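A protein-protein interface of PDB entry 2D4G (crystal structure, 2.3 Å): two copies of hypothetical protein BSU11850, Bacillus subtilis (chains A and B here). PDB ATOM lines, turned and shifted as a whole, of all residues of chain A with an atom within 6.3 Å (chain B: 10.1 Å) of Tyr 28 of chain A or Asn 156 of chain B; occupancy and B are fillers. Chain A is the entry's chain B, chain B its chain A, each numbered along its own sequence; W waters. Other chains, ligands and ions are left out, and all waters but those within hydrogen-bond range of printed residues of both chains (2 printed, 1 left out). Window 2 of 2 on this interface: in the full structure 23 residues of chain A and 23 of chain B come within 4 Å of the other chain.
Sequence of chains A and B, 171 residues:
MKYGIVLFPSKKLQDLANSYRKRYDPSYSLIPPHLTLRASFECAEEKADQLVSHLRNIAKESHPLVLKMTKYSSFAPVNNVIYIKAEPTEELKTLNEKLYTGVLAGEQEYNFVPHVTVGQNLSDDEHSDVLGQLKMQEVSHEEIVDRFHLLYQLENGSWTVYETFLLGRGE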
ATOM      1  N   ASP A  15     -13.660  24.519 -28.532  1.00  0.00           N
ATOM      2  CA  ASP A  15     -13.269  23.186 -28.975  1.00  0.00           C
ATOM      3  C   ASP A  15     -12.312  22.575 -27.961  1.00  0.00           C
ATOM      4  O   ASP A  15     -12.442  21.409 -27.595  1.00  0.00           O
ATOM      5  CB  ASP A  15     -12.599  23.241 -30.353  1.00  0.00           C
ATOM      6  CG  ASP A  15     -13.554  23.682 -31.454  1.00  0.00           C
ATOM      7  OD1 ASP A  15     -14.784  23.592 -31.255  1.00  0.00           O
ATOM      8  OD2 ASP A  15     -13.075  24.109 -32.526  1.00  0.00           O
ATOM      9  N   ASN A  18     -14.243  21.516 -25.030  1.00  0.00           N
ATOM     10  CA  ASN A  18     -15.106  20.381 -25.361  1.00  0.00           C
ATOM     11  C   ASN A  18     -14.376  19.054 -25.557  1.00  0.00           C
ATOM     12  O   ASN A  18     -14.994  17.988 -25.472  1.00  0.00           O
ATOM     13  CB  ASN A  18     -15.955  20.677 -26.606  1.00  0.00           C
ATOM     14  CG  ASN A  18     -17.257  21.386 -26.268  1.00  0.00           C
ATOM     15  OD1 ASN A  18     -17.737  21.314 -25.135  1.00  0.00           O
ATOM     16  ND2 ASN A  18     -17.851  22.053 -27.257  1.00  0.00           N
ATOM     17  N   SER A  19     -13.071  19.109 -25.820  1.00  0.00           N
ATOM     18  CA  SER A  19     -12.309  17.880 -26.014  1.00  0.00           C
ATOM     19  C   SER A  19     -12.239  17.141 -24.684  1.00  0.00           C
ATOM     20  O   SER A  19     -11.917  15.955 -24.639  1.00  0.00           O
ATOM     21  CB  SER A  19     -10.895  18.182 -26.534  1.00  0.00           C
ATOM     22  OG  SER A  19     -10.117  18.874 -25.572  1.00  0.00           O
ATOM     23  N   ARG A  21     -14.778  18.210 -22.024  1.00  0.00           N
ATOM     24  CA  ARG A  21     -16.158  18.264 -21.558  1.00  0.00           C
ATOM     25  C   ARG A  21     -16.992  17.085 -22.040  1.00  0.00           C
ATOM     26  O   ARG A  21     -17.873  16.600 -21.326  1.00  0.00           O
ATOM     27  CB  ARG A  21     -16.834  19.564 -22.014  1.00  0.00           C
ATOM     28  CG  ARG A  21     -16.365  20.822 -21.294  1.00  0.00           C
ATOM     29  CD  ARG A  21     -17.552  21.736 -21.017  1.00  0.00           C
ATOM     30  NE  ARG A  21     -18.290  22.022 -22.240  1.00  0.00           N
ATOM     31  CZ  ARG A  21     -19.561  22.404 -22.286  1.00  0.00           C
ATOM     32  NH1 ARG A  21     -20.261  22.551 -21.168  1.00  0.00           N
ATOM     33  NH2 ARG A  21     -20.137  22.636 -23.459  1.00  0.00           N
ATOM     34  N   LYS A  22     -16.717  16.624 -23.255  1.00  0.00           N
ATOM     35  CA  LYS A  22     -17.467  15.511 -23.826  1.00  0.00           C
ATOM     36  C   LYS A  22     -17.480  14.289 -22.913  1.00  0.00           C
ATOM     37  O   LYS A  22     -18.388  13.459 -22.994  1.00  0.00           O
ATOM     38  CB  LYS A  22     -16.894  15.135 -25.196  1.00  0.00           C
ATOM     39  CG  LYS A  22     -15.436  14.698 -25.177  1.00  0.00           C
ATOM     40  CD  LYS A  22     -14.890  14.582 -26.599  1.00  0.00           C
ATOM     41  CE  LYS A  22     -13.531  13.895 -26.624  1.00  0.00           C
ATOM     42  NZ  LYS A  22     -13.645  12.500 -26.109  1.00  0.00           N
ATOM     43  N   ARG A  23     -16.492  14.177 -22.031  1.00  0.00           N
ATOM     44  CA  ARG A  23     -16.458  13.023 -21.145  1.00  0.00           C
ATOM     45  C   ARG A  23     -16.563  13.304 -19.647  1.00  0.00           C
ATOM     46  O   ARG A  23     -16.881  12.399 -18.877  1.00  0.00           O
ATOM     47  CB  ARG A  23     -15.207  12.175 -21.437  1.00  0.00           C
ATOM     48  CG  ARG A  23     -13.883  12.847 -21.161  1.00  0.00           C
ATOM     49  CD  ARG A  23     -12.716  12.094 -21.812  1.00  0.00           C
ATOM     50  NE  ARG A  23     -12.743  10.653 -21.559  1.00  0.00           N
ATOM     51  CZ  ARG A  23     -11.656   9.892 -21.424  1.00  0.00           C
ATOM     52  NH1 ARG A  23     -10.443  10.428 -21.512  1.00  0.00           N
ATOM     53  NH2 ARG A  23     -11.780   8.586 -21.208  1.00  0.00           N
ATOM     54  N   ASP A  25     -18.100  16.517 -18.272  1.00  0.00           N
ATOM     55  CA  ASP A  25     -19.018  17.600 -17.926  1.00  0.00           C
ATOM     56  C   ASP A  25     -20.456  17.329 -18.358  1.00  0.00           C
ATOM     57  O   ASP A  25     -20.783  17.409 -19.542  1.00  0.00           O
ATOM     58  CB  ASP A  25     -18.536  18.911 -18.560  1.00  0.00           C
ATOM     59  CG  ASP A  25     -19.320  20.122 -18.077  1.00  0.00           C
ATOM     60  OD1 ASP A  25     -20.275  19.953 -17.290  1.00  0.00           O
ATOM     61  OD2 ASP A  25     -18.981  21.251 -18.488  1.00  0.00           O
ATOM     62  N   PRO A  26     -21.339  17.006 -17.397  1.00  0.00           N
ATOM     63  CA  PRO A  26     -22.740  16.736 -17.735  1.00  0.00           C
ATOM     64  C   PRO A  26     -23.403  17.889 -18.494  1.00  0.00           C
ATOM     65  O   PRO A  26     -24.403  17.688 -19.179  1.00  0.00           O
ATOM     66  CB  PRO A  26     -23.376  16.491 -16.372  1.00  0.00           C
ATOM     67  CG  PRO A  26     -22.260  15.801 -15.625  1.00  0.00           C
ATOM     68  CD  PRO A  26     -21.064  16.666 -15.987  1.00  0.00           C
ATOM     69  N   SER A  27     -22.845  19.093 -18.368  1.00  0.00           N
ATOM     70  CA  SER A  27     -23.390  20.263 -19.055  1.00  0.00           C
ATOM     71  C   SER A  27     -23.020  20.284 -20.530  1.00  0.00           C
ATOM     72  O   SER A  27     -23.499  21.131 -21.288  1.00  0.00           O
ATOM     73  CB  SER A  27     -22.898  21.549 -18.395  1.00  0.00           C
ATOM     74  OG  SER A  27     -23.571  21.768 -17.172  1.00  0.00           O
ATOM     75  N   TYR A  28     -22.175  19.342 -20.931  1.00  0.00           N
ATOM     76  CA  TYR A  28     -21.734  19.232 -22.311  1.00  0.00           C
ATOM     77  C   TYR A  28     -22.872  19.490 -23.294  1.00  0.00           C
ATOM     78  O   TYR A  28     -22.783  20.377 -24.145  1.00  0.00           O
ATOM     79  CB  TYR A  28     -21.147  17.840 -22.564  1.00  0.00           C
ATOM     80  CG  TYR A  28     -20.602  17.644 -23.962  1.00  0.00           C
ATOM     81  CD1 TYR A  28     -19.613  18.489 -24.468  1.00  0.00           C
ATOM     82  CD2 TYR A  28     -21.059  16.607 -24.774  1.00  0.00           C
ATOM     83  CE1 TYR A  28     -19.090  18.304 -25.743  1.00  0.00           C
ATOM     84  CE2 TYR A  28     -20.543  16.412 -26.059  1.00  0.00           C
ATOM     85  CZ  TYR A  28     -19.558  17.266 -26.532  1.00  0.00           C
ATOM     86  OH  TYR A  28     -19.036  17.080 -27.791  1.00  0.00           O
ATOM     87  N   SER A  29     -23.945  18.722 -23.166  1.00  0.00           N
ATOM     88  CA  SER A  29     -25.087  18.861 -24.062  1.00  0.00           C
ATOM     89  C   SER A  29     -26.091  19.913 -23.599  1.00  0.00           C
ATOM     90  O   SER A  29     -27.138  20.086 -24.222  1.00  0.00           O
ATOM     91  CB  SER A  29     -25.796  17.508 -24.205  1.00  0.00           C
ATOM     92  OG  SER A  29     -26.316  17.060 -22.958  1.00  0.00           O
ATOM     93  N   LEU A  30     -25.772  20.619 -22.517  1.00  0.00           N
ATOM     94  CA  LEU A  30     -26.674  21.633 -21.968  1.00  0.00           C
ATOM     95  C   LEU A  30     -26.394  23.071 -22.393  1.00  0.00           C
ATOM     96  O   LEU A  30     -27.320  23.869 -22.560  1.00  0.00           O
ATOM     97  CB  LEU A  30     -26.662  21.565 -20.436  1.00  0.00           C
ATOM     98  CG  LEU A  30     -27.573  20.546 -19.745  1.00  0.00           C
ATOM     99  CD1 LEU A  30     -27.546  19.206 -20.467  1.00  0.00           C
ATOM    100  CD2 LEU A  30     -27.127  20.393 -18.301  1.00  0.00           C
ATOM    101  N   ILE A  31     -25.118  23.399 -22.558  1.00  0.00           N
ATOM    102  CA  ILE A  31     -24.728  24.749 -22.925  1.00  0.00           C
ATOM    103  C   ILE A  31     -23.288  24.695 -23.423  1.00  0.00           C
ATOM    104  O   ILE A  31     -22.499  23.879 -22.950  1.00  0.00           O
ATOM    105  CB  ILE A  31     -24.829  25.672 -21.686  1.00  0.00           C
ATOM    106  CG1 ILE A  31     -24.486  27.115 -22.054  1.00  0.00           C
ATOM    107  CG2 ILE A  31     -23.906  25.160 -20.589  1.00  0.00           C
ATOM    108  CD1 ILE A  31     -24.593  28.072 -20.882  1.00  0.00           C
ATOM    109  N   PRO A  32     -22.931  25.553 -24.396  1.00  0.00           N
ATOM    110  CA  PRO A  32     -21.569  25.581 -24.943  1.00  0.00           C
ATOM    111  C   PRO A  32     -20.553  26.010 -23.891  1.00  0.00           C
ATOM    112  O   PRO A  32     -20.924  26.573 -22.864  1.00  0.00           O
ATOM    113  CB  PRO A  32     -21.671  26.607 -26.075  1.00  0.00           C
ATOM    114  CG  PRO A  32     -23.122  26.550 -26.467  1.00  0.00           C
ATOM    115  CD  PRO A  32     -23.807  26.476 -25.137  1.00  0.00           C
ATOM    116  N   GLN A 120     -17.263  18.418 -14.144  1.00  0.00           N
ATOM    117  CA  GLN A 120     -17.975  18.575 -12.872  1.00  0.00           C
ATOM    118  C   GLN A 120     -18.814  17.345 -12.505  1.00  0.00           C
ATOM    119  O   GLN A 120     -19.019  16.456 -13.335  1.00  0.00           O
ATOM    120  CB  GLN A 120     -18.854  19.829 -12.910  1.00  0.00           C
ATOM    121  CG  GLN A 120     -19.870  19.878 -14.040  1.00  0.00           C
ATOM    122  CD  GLN A 120     -20.549  21.235 -14.127  1.00  0.00           C
ATOM    123  OE1 GLN A 120     -20.714  21.915 -13.115  1.00  0.00           O
ATOM    124  NE2 GLN A 120     -20.958  21.629 -15.331  1.00  0.00           N
ATOM    125  N   PRO B  26     -30.793  13.652 -33.449  1.00  0.00           N
ATOM    126  CA  PRO B  26     -29.363  13.685 -33.125  1.00  0.00           C
ATOM    127  C   PRO B  26     -28.887  15.100 -32.799  1.00  0.00           C
ATOM    128  O   PRO B  26     -27.877  15.278 -32.122  1.00  0.00           O
ATOM    129  CB  PRO B  26     -28.707  13.128 -34.390  1.00  0.00           C
ATOM    130  CG  PRO B  26     -29.744  12.197 -34.919  1.00  0.00           C
ATOM    131  CD  PRO B  26     -31.015  13.003 -34.753  1.00  0.00           C
ATOM    132  N   SER B  27     -29.618  16.104 -33.280  1.00  0.00           N
ATOM    133  CA  SER B  27     -29.262  17.494 -33.013  1.00  0.00           C
ATOM    134  C   SER B  27     -29.635  17.883 -31.593  1.00  0.00           C
ATOM    135  O   SER B  27     -29.289  18.968 -31.124  1.00  0.00           O
ATOM    136  CB  SER B  27     -29.975  18.438 -33.987  1.00  0.00           C
ATOM    137  OG  SER B  27     -29.523  18.253 -35.314  1.00  0.00           O
ATOM    138  N   TYR B  28     -30.353  16.999 -30.910  1.00  0.00           N
ATOM    139  CA  TYR B  28     -30.774  17.268 -29.544  1.00  0.00           C
ATOM    140  C   TYR B  28     -29.672  17.918 -28.712  1.00  0.00           C
ATOM    141  O   TYR B  28     -29.888  18.949 -28.084  1.00  0.00           O
ATOM    142  CB  TYR B  28     -31.215  15.976 -28.860  1.00  0.00           C
ATOM    143  CG  TYR B  28     -31.690  16.181 -27.442  1.00  0.00           C
ATOM    144  CD1 TYR B  28     -32.751  17.040 -27.171  1.00  0.00           C
ATOM    145  CD2 TYR B  28     -31.104  15.492 -26.377  1.00  0.00           C
ATOM    146  CE1 TYR B  28     -33.227  17.210 -25.886  1.00  0.00           C
ATOM    147  CE2 TYR B  28     -31.579  15.658 -25.070  1.00  0.00           C
ATOM    148  CZ  TYR B  28     -32.648  16.522 -24.843  1.00  0.00           C
ATOM    149  OH  TYR B  28     -33.184  16.708 -23.591  1.00  0.00           O
ATOM    150  N   SER B  29     -28.491  17.313 -28.714  1.00  0.00           N
ATOM    151  CA  SER B  29     -27.368  17.828 -27.933  1.00  0.00           C
ATOM    152  C   SER B  29     -26.521  18.863 -28.668  1.00  0.00           C
ATOM    153  O   SER B  29     -25.517  19.333 -28.138  1.00  0.00           O
ATOM    154  CB  SER B  29     -26.468  16.665 -27.492  1.00  0.00           C
ATOM    155  OG  SER B  29     -25.921  15.977 -28.609  1.00  0.00           O
ATOM    156  N   LEU B  30     -26.938  19.238 -29.873  1.00  0.00           N
ATOM    157  CA  LEU B  30     -26.181  20.193 -30.675  1.00  0.00           C
ATOM    158  C   LEU B  30     -26.757  21.597 -30.740  1.00  0.00           C
ATOM    159  O   LEU B  30     -26.037  22.551 -31.034  1.00  0.00           O
ATOM    160  CB  LEU B  30     -26.048  19.675 -32.109  1.00  0.00           C
ATOM    161  CG  LEU B  30     -25.431  18.293 -32.316  1.00  0.00           C
ATOM    162  CD1 LEU B  30     -25.313  18.022 -33.807  1.00  0.00           C
ATOM    163  CD2 LEU B  30     -24.071  18.223 -31.645  1.00  0.00           C
ATOM    164  N   ILE B  31     -28.052  21.726 -30.478  1.00  0.00           N
ATOM    165  CA  ILE B  31     -28.705  23.023 -30.562  1.00  0.00           C
ATOM    166  C   ILE B  31     -30.153  22.894 -30.090  1.00  0.00           C
ATOM    167  O   ILE B  31     -30.803  21.878 -30.333  1.00  0.00           O
ATOM    168  CB  ILE B  31     -28.683  23.521 -32.030  1.00  0.00           C
ATOM    169  CG1 ILE B  31     -29.295  24.919 -32.138  1.00  0.00           C
ATOM    170  CG2 ILE B  31     -29.438  22.543 -32.908  1.00  0.00           C
ATOM    171  CD1 ILE B  31     -29.380  25.443 -33.555  1.00  0.00           C
ATOM    172  N   PRO B  32     -30.675  23.919 -29.399  1.00  0.00           N
ATOM    173  CA  PRO B  32     -32.062  23.861 -28.919  1.00  0.00           C
ATOM    174  C   PRO B  32     -33.088  23.978 -30.053  1.00  0.00           C
ATOM    175  O   PRO B  32     -32.758  24.422 -31.152  1.00  0.00           O
ATOM    176  CB  PRO B  32     -32.135  25.022 -27.929  1.00  0.00           C
ATOM    177  CG  PRO B  32     -31.142  26.007 -28.480  1.00  0.00           C
ATOM    178  CD  PRO B  32     -29.987  25.120 -28.891  1.00  0.00           C
ATOM    179  N   TYR B 152     -22.541  29.822 -35.242  1.00  0.00           N
ATOM    180  CA  TYR B 152     -21.472  29.135 -35.969  1.00  0.00           C
ATOM    181  C   TYR B 152     -21.251  27.754 -35.354  1.00  0.00           C
ATOM    182  O   TYR B 152     -21.505  27.544 -34.163  1.00  0.00           O
ATOM    183  CB  TYR B 152     -20.181  29.957 -35.926  1.00  0.00           C
ATOM    184  CG  TYR B 152     -19.733  30.325 -34.533  1.00  0.00           C
ATOM    185  CD1 TYR B 152     -18.883  29.493 -33.807  1.00  0.00           C
ATOM    186  CD2 TYR B 152     -20.181  31.501 -33.927  1.00  0.00           C
ATOM    187  CE1 TYR B 152     -18.488  29.822 -32.509  1.00  0.00           C
ATOM    188  CE2 TYR B 152     -19.795  31.840 -32.626  1.00  0.00           C
ATOM    189  CZ  TYR B 152     -18.949  30.998 -31.925  1.00  0.00           C
ATOM    190  OH  TYR B 152     -18.568  31.335 -30.642  1.00  0.00           O
ATOM    191  N   GLN B 153     -20.755  26.823 -36.162  1.00  0.00           N
ATOM    192  CA  GLN B 153     -20.556  25.445 -35.739  1.00  0.00           C
ATOM    193  C   GLN B 153     -19.208  25.092 -35.135  1.00  0.00           C
ATOM    194  O   GLN B 153     -18.157  25.408 -35.696  1.00  0.00           O
ATOM    195  CB  GLN B 153     -20.830  24.538 -36.931  1.00  0.00           C
ATOM    196  CG  GLN B 153     -20.855  23.065 -36.635  1.00  0.00           C
ATOM    197  CD  GLN B 153     -21.310  22.277 -37.840  1.00  0.00           C
ATOM    198  OE1 GLN B 153     -20.649  22.277 -38.881  1.00  0.00           O
ATOM    199  NE2 GLN B 153     -22.449  21.610 -37.714  1.00  0.00           N
ATOM    200  N   LEU B 154     -19.245  24.421 -33.987  1.00  0.00           N
ATOM    201  CA  LEU B 154     -18.021  23.996 -33.323  1.00  0.00           C
ATOM    202  C   LEU B 154     -17.514  22.712 -33.932  1.00  0.00           C
ATOM    203  O   LEU B 154     -18.174  22.092 -34.761  1.00  0.00           O
ATOM    204  CB  LEU B 154     -18.259  23.751 -31.837  1.00  0.00           C
ATOM    205  CG  LEU B 154     -18.713  24.959 -31.022  1.00  0.00           C
ATOM    206  CD1 LEU B 154     -18.640  24.604 -29.538  1.00  0.00           C
ATOM    207  CD2 LEU B 154     -17.747  26.115 -31.262  1.00  0.00           C
ATOM    208  N   GLU B 155     -16.325  22.318 -33.510  1.00  0.00           N
ATOM    209  CA  GLU B 155     -15.717  21.100 -34.000  1.00  0.00           C
ATOM    210  C   GLU B 155     -16.658  19.919 -33.787  1.00  0.00           C
ATOM    211  O   GLU B 155     -16.854  19.108 -34.688  1.00  0.00           O
ATOM    212  CB  GLU B 155     -14.396  20.861 -33.269  1.00  0.00           C
ATOM    213  CG  GLU B 155     -13.642  19.630 -33.716  1.00  0.00           C
ATOM    214  CD  GLU B 155     -12.236  19.590 -33.162  1.00  0.00           C
ATOM    215  OE1 GLU B 155     -11.309  19.263 -33.935  1.00  0.00           O
ATOM    216  OE2 GLU B 155     -12.052  19.885 -31.958  1.00  0.00           O
ATOM    217  N   ASN B 156     -17.264  19.839 -32.605  1.00  0.00           N
ATOM    218  CA  ASN B 156     -18.154  18.722 -32.302  1.00  0.00           C
ATOM    219  C   ASN B 156     -19.538  18.791 -32.941  1.00  0.00           C
ATOM    220  O   ASN B 156     -20.419  18.000 -32.600  1.00  0.00           O
ATOM    221  CB  ASN B 156     -18.303  18.545 -30.785  1.00  0.00           C
ATOM    222  CG  ASN B 156     -19.223  19.575 -30.155  1.00  0.00           C
ATOM    223  OD1 ASN B 156     -19.536  19.484 -28.963  1.00  0.00           O
ATOM    224  ND2 ASN B 156     -19.665  20.554 -30.943  1.00  0.00           N
ATOM    225  N   GLY B 157     -19.731  19.732 -33.860  1.00  0.00           N
ATOM    226  CA  GLY B 157     -21.014  19.853 -34.534  1.00  0.00           C
ATOM    227  C   GLY B 157     -22.070  20.724 -33.868  1.00  0.00           C
ATOM    228  O   GLY B 157     -23.045  21.113 -34.519  1.00  0.00           O
ATOM    229  N   SER B 158     -21.913  21.030 -32.582  1.00  0.00           N
ATOM    230  CA  SER B 158     -22.907  21.867 -31.911  1.00  0.00           C
ATOM    231  C   SER B 158     -22.803  23.290 -32.438  1.00  0.00           C
ATOM    232  O   SER B 158     -21.803  23.653 -33.055  1.00  0.00           O
ATOM    233  CB  SER B 158     -22.708  21.847 -30.391  1.00  0.00           C
ATOM    234  OG  SER B 158     -21.436  22.334 -30.021  1.00  0.00           O
ATOM    235  N   TRP B 159     -23.846  24.085 -32.209  1.00  0.00           N
ATOM    236  CA  TRP B 159     -23.884  25.468 -32.671  1.00  0.00           C
ATOM    237  C   TRP B 159     -23.935  26.467 -31.510  1.00  0.00           C
ATOM    238  O   TRP B 159     -24.675  26.270 -30.547  1.00  0.00           O
ATOM    239  CB  TRP B 159     -25.102  25.689 -33.581  1.00  0.00           C
ATOM    240  CG  TRP B 159     -25.110  24.834 -34.831  1.00  0.00           C
ATOM    241  CD1 TRP B 159     -25.453  23.513 -34.922  1.00  0.00           C
ATOM    242  CD2 TRP B 159     -24.785  25.262 -36.164  1.00  0.00           C
ATOM    243  NE1 TRP B 159     -25.334  23.073 -36.223  1.00  0.00           N
ATOM    244  CE2 TRP B 159     -24.896  24.094 -36.983  1.00  0.00           C
ATOM    245  CE3 TRP B 159     -24.315  26.453 -36.708  1.00  0.00           C
ATOM    246  CZ2 TRP B 159     -24.667  24.173 -38.367  1.00  0.00           C
ATOM    247  CZ3 TRP B 159     -24.081  26.505 -38.074  1.00  0.00           C
ATOM    248  CH2 TRP B 159     -24.212  25.359 -38.878  1.00  0.00           C
ATOM    249  N   THR B 160     -23.146  27.537 -31.615  1.00  0.00           N
ATOM    250  CA  THR B 160     -23.091  28.588 -30.601  1.00  0.00           C
ATOM    251  C   THR B 160     -23.606  29.900 -31.199  1.00  0.00           C
ATOM    252  O   THR B 160     -23.357  30.188 -32.366  1.00  0.00           O
ATOM    253  CB  THR B 160     -21.645  28.834 -30.108  1.00  0.00           C
ATOM    254  OG1 THR B 160     -21.111  27.632 -29.535  1.00  0.00           O
ATOM    255  CG2 THR B 160     -21.620  29.955 -29.069  1.00  0.00           C
HETATM  256  O   HOH W   1     -20.874  23.223 -27.014  1.00  0.00           O
HETATM  257  O   HOH W   2     -14.219  19.697 -29.785  1.00  0.00           O
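The side-chain amide oxygen (OD1) of Asn 156 of chain B is in hydrogen-bond range of the side-chain hydroxyl (OH) of Tyr 28 of chain A.
The side-chain carboxylate (OD1) of Asp 15 of chain A is in hydrogen-bond range of the backbone NH (N) of Glu 155 of chain B, at 3.0 Å.
N of Tyr 152 of chain B is in hydrogen-bond range of O of Thr 160 of chain B, at 3.0 Å.
The side-chain amide nitrogen (ND2) of Asn 156 of chain B is in hydrogen-bond range of the side-chain hydroxyl (OG) of Ser 158 of chain B, at 2.7 Å.
The side-chain amide oxygen (OD1) of Asn 18 of chain A lies within hydrogen-bond range of the guanidinium group (NE) of Arg 21 of chain A, 3.0 Å away.
Among the printed residues, pairs that only touch across the chains: Asp 15 of chain A with Leu 154 of chain B (3.5 Å), Asn 18 of chain A with Leu 154 of chain B (3.5 Å), Asn 18 of chain A with Asn 156 of chain B (3.5 Å), Ser 29 of chain A with Ser 29 of chain B (3.5 Å) and Pro 32 of chain A with Thr 160 of chain B (3.7 Å).
Of the printed residues of chain B, Asp 15 of chain A touches Leu 154 and Glu 155.
No residue of chain B comes within 4 Å of Arg 21 of chain A.
No residue of chain B comes within 4 Å of Asp 25 of chain A.
Of the printed residues of chain B, Tyr 28 of chain A touches Asn 156 (2.7 Å).
Ser 29 of chain A touches just one residue of chain B: Ser 29.
No residue of chain B comes within 4 Å of Leu 30 of chain A.
Printed residues of chain A within 4 Å of Ser 29 of chain B: Ser 29.
Ile 31 of chain B touches none of the printed residues of chain A.
Of chain A, only Asn 18 and Tyr 28 come within 4 Å of Asn 156 of chain B.
Trp 159 of chain B touches none of the printed residues of chain A.
The nearest residue of chain B that does not touch Tyr 28 of chain A is Ser 29 of chain B (5.0 Å).
The nearest residue of chain A that does not touch Asn 156 of chain B is Asp 15 of chain A (4.7 Å).
The nearest printed residue of chain B that does not touch Pro 32 of chain A is Trp 159 of chain B (4.4 Å).
Of the 16 printed residues of chain B, 5 touch a printed residue of chain A.
Printed residues of chain B that touch a printed residue of chain A: Ser 29, Leu 154, Glu 155, Asn 156 and Thr 160.
Hydrophobic or aromatic side chains of chain A that line the printed part of chain B: Tyr 28 and Pro 32.
Among the printed residues, no Asp or Glu carboxylate lies within 4 Å of a Lys or Arg side-chain nitrogen of the other chain.
Ser 29 of chain A touches its own counterpart, Ser 29 of chain B.
Positions printed for both chains: 26, 27, 28, 29, 30, 31 and 32.
Water W2 bridges the side-chain carboxylate (OE2) of Glu 155 of chain B (3.1 Å) and the backbone carbonyl oxygen (O) of Asp 15 of chain A (3.3 Å).
Water W1 lies within hydrogen-bond range of OG of Ser 158 of chain B (3.2 Å) and ND2 of Asn 18 of chain A (3.3 Å).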
